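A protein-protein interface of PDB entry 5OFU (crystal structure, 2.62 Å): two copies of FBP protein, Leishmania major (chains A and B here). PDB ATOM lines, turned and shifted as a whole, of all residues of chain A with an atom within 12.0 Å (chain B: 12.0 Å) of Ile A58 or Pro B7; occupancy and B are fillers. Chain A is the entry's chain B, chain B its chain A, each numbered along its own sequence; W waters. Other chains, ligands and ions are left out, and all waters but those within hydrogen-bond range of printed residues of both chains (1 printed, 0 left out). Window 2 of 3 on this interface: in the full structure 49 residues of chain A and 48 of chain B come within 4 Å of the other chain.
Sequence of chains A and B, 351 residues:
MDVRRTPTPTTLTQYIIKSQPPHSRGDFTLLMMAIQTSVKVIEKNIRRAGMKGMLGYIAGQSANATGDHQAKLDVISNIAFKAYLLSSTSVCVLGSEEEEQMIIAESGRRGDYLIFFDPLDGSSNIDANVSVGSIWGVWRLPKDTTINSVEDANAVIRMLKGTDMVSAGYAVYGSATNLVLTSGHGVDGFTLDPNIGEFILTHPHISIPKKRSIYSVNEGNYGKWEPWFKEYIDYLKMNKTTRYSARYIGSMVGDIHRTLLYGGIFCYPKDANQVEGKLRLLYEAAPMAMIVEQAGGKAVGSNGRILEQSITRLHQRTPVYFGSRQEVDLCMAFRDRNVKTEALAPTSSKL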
ATOM      1  N   ARG A  48       6.009 -34.585  14.235  1.00  0.00           N
ATOM      2  CA  ARG A  48       6.289 -33.810  15.433  1.00  0.00           C
ATOM      3  C   ARG A  48       7.730 -33.913  15.927  1.00  0.00           C
ATOM      4  O   ARG A  48       8.050 -33.299  16.933  1.00  0.00           O
ATOM      5  CB  ARG A  48       5.422 -34.286  16.584  1.00  0.00           C
ATOM      6  CG  ARG A  48       3.942 -34.081  16.416  1.00  0.00           C
ATOM      7  CD  ARG A  48       3.267 -34.422  17.740  1.00  0.00           C
ATOM      8  NE  ARG A  48       3.764 -33.504  18.762  1.00  0.00           N
ATOM      9  CZ  ARG A  48       3.392 -32.233  18.880  1.00  0.00           C
ATOM     10  NH1 ARG A  48       2.466 -31.721  18.072  1.00  0.00           N
ATOM     11  NH2 ARG A  48       3.938 -31.471  19.826  1.00  0.00           N
ATOM     12  N   MET A  51       8.256 -34.176  19.745  1.00  0.00           N
ATOM     13  CA  MET A  51       7.962 -33.105  20.716  1.00  0.00           C
ATOM     14  C   MET A  51       6.729 -33.477  21.527  1.00  0.00           C
ATOM     15  O   MET A  51       5.757 -34.008  20.976  1.00  0.00           O
ATOM     16  CB  MET A  51       7.654 -31.777  20.028  1.00  0.00           C
ATOM     17  CG  MET A  51       8.821 -31.114  19.325  1.00  0.00           C
ATOM     18  SD  MET A  51       8.373 -29.534  18.582  1.00  0.00           S
ATOM     19  CE  MET A  51       7.139 -29.976  17.356  1.00  0.00           C
ATOM     20  N   LYS A  52       6.784 -33.229  22.831  1.00  0.00           N
ATOM     21  CA  LYS A  52       5.598 -33.331  23.675  1.00  0.00           C
ATOM     22  C   LYS A  52       4.596 -32.270  23.240  1.00  0.00           C
ATOM     23  O   LYS A  52       4.979 -31.261  22.646  1.00  0.00           O
ATOM     24  CB  LYS A  52       5.945 -33.115  25.149  1.00  0.00           C
ATOM     25  CG  LYS A  52       6.383 -34.360  25.910  1.00  0.00           C
ATOM     26  CD  LYS A  52       6.517 -34.052  27.458  1.00  0.00           C
ATOM     27  CE  LYS A  52       7.781 -33.453  28.022  1.00  0.00           C
ATOM     28  NZ  LYS A  52       8.281 -32.296  27.240  1.00  0.00           N
ATOM     29  N   GLY A  53       3.313 -32.510  23.515  1.00  0.00           N
ATOM     30  CA  GLY A  53       2.287 -31.480  23.347  1.00  0.00           C
ATOM     31  C   GLY A  53       2.589 -30.328  24.288  1.00  0.00           C
ATOM     32  O   GLY A  53       3.288 -30.507  25.289  1.00  0.00           O
ATOM     33  N   MET A  54       2.057 -29.150  23.975  1.00  0.00           N
ATOM     34  CA  MET A  54       2.328 -27.940  24.772  1.00  0.00           C
ATOM     35  C   MET A  54       1.816 -28.077  26.218  1.00  0.00           C
ATOM     36  O   MET A  54       2.300 -27.416  27.141  1.00  0.00           O
ATOM     37  CB  MET A  54       1.734 -26.695  24.097  1.00  0.00           C
ATOM     38  CG  MET A  54       2.205 -26.433  22.664  1.00  0.00           C
ATOM     39  SD  MET A  54       3.979 -26.175  22.433  1.00  0.00           S
ATOM     40  CE  MET A  54       4.601 -27.816  22.043  1.00  0.00           C
ATOM     41  N   LEU A  55       0.832 -28.943  26.404  1.00  0.00           N
ATOM     42  CA  LEU A  55       0.429 -29.376  27.731  1.00  0.00           C
ATOM     43  C   LEU A  55       1.487 -30.261  28.427  1.00  0.00           C
ATOM     44  O   LEU A  55       1.789 -30.051  29.601  1.00  0.00           O
ATOM     45  CB  LEU A  55      -0.921 -30.066  27.654  1.00  0.00           C
ATOM     46  CG  LEU A  55      -2.260 -29.446  27.437  1.00  0.00           C
ATOM     47  CD1 LEU A  55      -2.116 -28.054  26.901  1.00  0.00           C
ATOM     48  CD2 LEU A  55      -3.134 -30.324  26.534  1.00  0.00           C
ATOM     49  N   GLY A  56       2.040 -31.242  27.712  1.00  0.00           N
ATOM     50  CA  GLY A  56       3.118 -32.089  28.215  1.00  0.00           C
ATOM     51  C   GLY A  56       4.371 -31.362  28.699  1.00  0.00           C
ATOM     52  O   GLY A  56       5.082 -31.835  29.601  1.00  0.00           O
ATOM     53  N   TYR A  57       4.665 -30.229  28.068  1.00  0.00           N
ATOM     54  CA  TYR A  57       5.819 -29.403  28.435  1.00  0.00           C
ATOM     55  C   TYR A  57       5.667 -28.674  29.752  1.00  0.00           C
ATOM     56  O   TYR A  57       6.647 -28.544  30.488  1.00  0.00           O
ATOM     57  CB  TYR A  57       6.113 -28.398  27.327  1.00  0.00           C
ATOM     58  CG  TYR A  57       7.382 -27.562  27.474  1.00  0.00           C
ATOM     59  CD1 TYR A  57       7.416 -26.397  28.263  1.00  0.00           C
ATOM     60  CD2 TYR A  57       8.544 -27.921  26.791  1.00  0.00           C
ATOM     61  CE1 TYR A  57       8.577 -25.641  28.375  1.00  0.00           C
ATOM     62  CE2 TYR A  57       9.708 -27.170  26.896  1.00  0.00           C
ATOM     63  CZ  TYR A  57       9.721 -26.035  27.688  1.00  0.00           C
ATOM     64  OH  TYR A  57      10.878 -25.298  27.785  1.00  0.00           O
ATOM     65  N   ILE A  58       4.473 -28.150  30.029  1.00  0.00           N
ATOM     66  CA  ILE A  58       4.233 -27.530  31.339  1.00  0.00           C
ATOM     67  C   ILE A  58       4.242 -28.533  32.495  1.00  0.00           C
ATOM     68  O   ILE A  58       4.735 -28.204  33.564  1.00  0.00           O
ATOM     69  CB  ILE A  58       2.997 -26.622  31.402  1.00  0.00           C
ATOM     70  CG1 ILE A  58       3.003 -25.832  32.730  1.00  0.00           C
ATOM     71  CG2 ILE A  58       1.722 -27.412  31.202  1.00  0.00           C
ATOM     72  CD1 ILE A  58       2.118 -24.615  32.744  1.00  0.00           C
ATOM     73  N   ALA A  59       3.699 -29.732  32.278  1.00  0.00           N
ATOM     74  CA  ALA A  59       3.741 -30.796  33.294  1.00  0.00           C
ATOM     75  C   ALA A  59       5.179 -31.261  33.636  1.00  0.00           C
ATOM     76  O   ALA A  59       5.433 -31.698  34.758  1.00  0.00           O
ATOM     77  CB  ALA A  59       2.873 -31.976  32.866  1.00  0.00           C
ATOM     78  N   GLY A  60       6.111 -31.140  32.688  1.00  0.00           N
ATOM     79  CA  GLY A  60       7.519 -31.492  32.922  1.00  0.00           C
ATOM     80  C   GLY A  60       8.254 -30.498  33.812  1.00  0.00           C
ATOM     81  O   GLY A  60       8.038 -29.287  33.730  1.00  0.00           O
ATOM     82  N   PRO B   7       8.623 -22.436  31.292  1.00  0.00           N
ATOM     83  CA  PRO B   7       7.179 -22.407  31.552  1.00  0.00           C
ATOM     84  C   PRO B   7       6.349 -22.937  30.363  1.00  0.00           C
ATOM     85  O   PRO B   7       5.645 -23.943  30.509  1.00  0.00           O
ATOM     86  CB  PRO B   7       6.903 -20.916  31.844  1.00  0.00           C
ATOM     87  CG  PRO B   7       8.142 -20.164  31.411  1.00  0.00           C
ATOM     88  CD  PRO B   7       9.128 -21.133  30.830  1.00  0.00           C
ATOM     89  N   THR B   8       6.431 -22.249  29.218  1.00  0.00           N
ATOM     90  CA  THR B   8       5.951 -22.742  27.919  1.00  0.00           C
ATOM     91  C   THR B   8       7.115 -22.655  26.929  1.00  0.00           C
ATOM     92  O   THR B   8       8.031 -21.855  27.119  1.00  0.00           O
ATOM     93  CB  THR B   8       4.774 -21.908  27.361  1.00  0.00           C
ATOM     94  OG1 THR B   8       5.218 -20.585  27.025  1.00  0.00           O
ATOM     95  CG2 THR B   8       3.634 -21.815  28.370  1.00  0.00           C
ATOM     96  N   PRO B   9       7.092 -23.470  25.866  1.00  0.00           N
ATOM     97  CA  PRO B   9       8.210 -23.421  24.920  1.00  0.00           C
ATOM     98  C   PRO B   9       8.130 -22.201  23.998  1.00  0.00           C
ATOM     99  O   PRO B   9       7.042 -21.753  23.672  1.00  0.00           O
ATOM    100  CB  PRO B   9       8.066 -24.732  24.137  1.00  0.00           C
ATOM    101  CG  PRO B   9       6.615 -25.016  24.179  1.00  0.00           C
ATOM    102  CD  PRO B   9       6.103 -24.501  25.495  1.00  0.00           C
ATOM    103  N   THR B  10       9.288 -21.702  23.580  1.00  0.00           N
ATOM    104  CA  THR B  10       9.402 -20.488  22.777  1.00  0.00           C
ATOM    105  C   THR B  10       9.009 -20.707  21.323  1.00  0.00           C
ATOM    106  O   THR B  10       9.549 -21.581  20.670  1.00  0.00           O
ATOM    107  CB  THR B  10      10.862 -19.997  22.775  1.00  0.00           C
ATOM    108  OG1 THR B  10      11.334 -19.928  24.119  1.00  0.00           O
ATOM    109  CG2 THR B  10      10.984 -18.623  22.116  1.00  0.00           C
ATOM    110  N   THR B  11       8.089 -19.899  20.814  1.00  0.00           N
ATOM    111  CA  THR B  11       7.726 -19.956  19.403  1.00  0.00           C
ATOM    112  C   THR B  11       8.674 -19.081  18.580  1.00  0.00           C
ATOM    113  O   THR B  11       9.321 -18.201  19.120  1.00  0.00           O
ATOM    114  CB  THR B  11       6.276 -19.499  19.177  1.00  0.00           C
ATOM    115  OG1 THR B  11       6.132 -18.123  19.554  1.00  0.00           O
ATOM    116  CG2 THR B  11       5.315 -20.357  19.995  1.00  0.00           C
ATOM    117  N   GLN B  14       7.516 -15.306  18.941  1.00  0.00           N
ATOM    118  CA  GLN B  14       8.124 -14.718  20.150  1.00  0.00           C
ATOM    119  C   GLN B  14       9.597 -14.389  19.988  1.00  0.00           C
ATOM    120  O   GLN B  14      10.035 -13.285  20.315  1.00  0.00           O
ATOM    121  CB  GLN B  14       8.012 -15.659  21.342  1.00  0.00           C
ATOM    122  CG  GLN B  14       6.679 -15.577  22.056  1.00  0.00           C
ATOM    123  CD  GLN B  14       6.311 -16.855  22.787  1.00  0.00           C
ATOM    124  OE1 GLN B  14       7.106 -17.802  22.889  1.00  0.00           O
ATOM    125  NE2 GLN B  14       5.081 -16.897  23.297  1.00  0.00           N
ATOM    126  N   LYS B  18      11.164 -10.676  20.341  1.00  0.00           N
ATOM    127  CA  LYS B  18      12.130 -10.465  21.431  1.00  0.00           C
ATOM    128  C   LYS B  18      13.549 -10.159  20.969  1.00  0.00           C
ATOM    129  O   LYS B  18      14.322  -9.608  21.736  1.00  0.00           O
ATOM    130  CB  LYS B  18      12.138 -11.646  22.413  1.00  0.00           C
ATOM    131  CG  LYS B  18      10.979 -11.586  23.391  1.00  0.00           C
ATOM    132  CD  LYS B  18      10.774 -12.894  24.140  1.00  0.00           C
ATOM    133  CE  LYS B  18       9.517 -12.828  24.998  1.00  0.00           C
ATOM    134  NZ  LYS B  18       9.156 -14.161  25.552  1.00  0.00           N
ATOM    135  N   ASP B 193       5.258 -27.485  14.760  1.00  0.00           N
ATOM    136  CA  ASP B 193       4.289 -28.276  15.469  1.00  0.00           C
ATOM    137  C   ASP B 193       3.005 -28.200  14.633  1.00  0.00           C
ATOM    138  O   ASP B 193       2.360 -27.156  14.611  1.00  0.00           O
ATOM    139  CB  ASP B 193       4.091 -27.697  16.861  1.00  0.00           C
ATOM    140  CG  ASP B 193       3.114 -28.492  17.702  1.00  0.00           C
ATOM    141  OD1 ASP B 193       2.283 -29.250  17.151  1.00  0.00           O
ATOM    142  OD2 ASP B 193       3.168 -28.330  18.943  1.00  0.00           O
ATOM    143  N   ILE B 196      -0.784 -27.043  16.182  1.00  0.00           N
ATOM    144  CA  ILE B 196      -1.070 -25.628  16.387  1.00  0.00           C
ATOM    145  C   ILE B 196      -0.448 -24.708  15.332  1.00  0.00           C
ATOM    146  O   ILE B 196      -0.608 -23.486  15.407  1.00  0.00           O
ATOM    147  CB  ILE B 196      -0.647 -25.181  17.814  1.00  0.00           C
ATOM    148  CG1 ILE B 196       0.873 -25.285  18.040  1.00  0.00           C
ATOM    149  CG2 ILE B 196      -1.370 -26.023  18.854  1.00  0.00           C
ATOM    150  CD1 ILE B 196       1.341 -24.715  19.364  1.00  0.00           C
ATOM    151  N   ILE B 200       8.446 -24.140  16.904  1.00  0.00           N
ATOM    152  CA  ILE B 200       8.852 -24.208  18.318  1.00  0.00           C
ATOM    153  C   ILE B 200      10.365 -24.350  18.349  1.00  0.00           C
ATOM    154  O   ILE B 200      10.924 -25.112  17.573  1.00  0.00           O
ATOM    155  CB  ILE B 200       8.173 -25.398  19.058  1.00  0.00           C
ATOM    156  CG1 ILE B 200       6.776 -25.015  19.558  1.00  0.00           C
ATOM    157  CG2 ILE B 200       8.943 -25.826  20.301  1.00  0.00           C
ATOM    158  CD1 ILE B 200       5.832 -24.524  18.492  1.00  0.00           C
ATOM    159  N   LEU B 201      11.020 -23.616  19.245  1.00  0.00           N
ATOM    160  CA  LEU B 201      12.472 -23.647  19.384  1.00  0.00           C
ATOM    161  C   LEU B 201      12.898 -24.999  19.930  1.00  0.00           C
ATOM    162  O   LEU B 201      12.634 -25.307  21.084  1.00  0.00           O
ATOM    163  CB  LEU B 201      12.939 -22.533  20.324  1.00  0.00           C
ATOM    164  CG  LEU B 201      14.445 -22.424  20.594  1.00  0.00           C
ATOM    165  CD1 LEU B 201      15.243 -22.343  19.304  1.00  0.00           C
ATOM    166  CD2 LEU B 201      14.725 -21.200  21.454  1.00  0.00           C
HETATM  167  O   HOH W   1       0.895 -29.579  20.347  1.00  0.00           O
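The guanidinium group (NH1) of Arg A48 lies within salt-bridge range of the side-chain carboxylate (OD1) of Asp B193 (2.6 Å).
NE of Arg A48 is in hydrogen-bond range of O of Met A51.
O of Lys A52 is in hydrogen-bond range of NH2 of Arg A48, at 3.0 Å.
Among the printed residues, pairs that only touch across the chains: Met A54 with Pro B9, Met A54 with Asp B193, Tyr A57 with Pro B9, Tyr A57 with Thr B8, Tyr A57 with Pro B7, Met A51 with Asp B193, Met A54 with Ile B196 and Ile A58 with Pro B7.
Printed residues of chain B within 4 Å of Arg A48: Asp B193.
Gly A53 touches none of the printed residues of chain B.
Of the printed residues of chain B, Met A54 touches Pro B9, Asp B193 and Ile B196.
Leu A55 touches none of the printed residues of chain B.
No residue of chain B comes within 4 Å of Gly A56.
Tyr A57 touches just these residues of chain B: Pro B7 (3.8 Å), Thr B8 (3.6 Å) and Pro B9 (3.6 Å).
Of chain B, only Pro B7 comes within 4 Å of Ile A58.
No residue of chain B comes within 4 Å of Ala A59.
No residue of chain B comes within 4 Å of Gly A60.
Thr B8 touches one residue of chain A.
Pro B9 touches two residues of chain A.
Of the printed residues of chain A, Asp B193 touches Arg A48, Met A51 and Met A54.
Printed residues of chain A within 4 Å of Ile B196: Met A54.
The nearest residue of chain A that does not touch Pro B7 is Met A54 (5.9 Å).
Of the 11 printed residues of chain A, 5 touch a printed residue of chain B.
Printed residues of chain A that touch a printed residue of chain B: Arg A48, Met A51, Met A54, Tyr A57 and Ile A58.
Along chain A the printed residues that touch a printed residue of chain B span positions 48 to 58.
Among the printed residues, Asp or Glu carboxylates within 4 Å of a Lys or Arg side-chain nitrogen of the other chain: Arg A48 with Asp B193.
No position is printed for both chains.
Water W1 bridges the side-chain carboxylate (OD2) of Asp B193 and the guanidinium group (NH1) of Arg A48.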
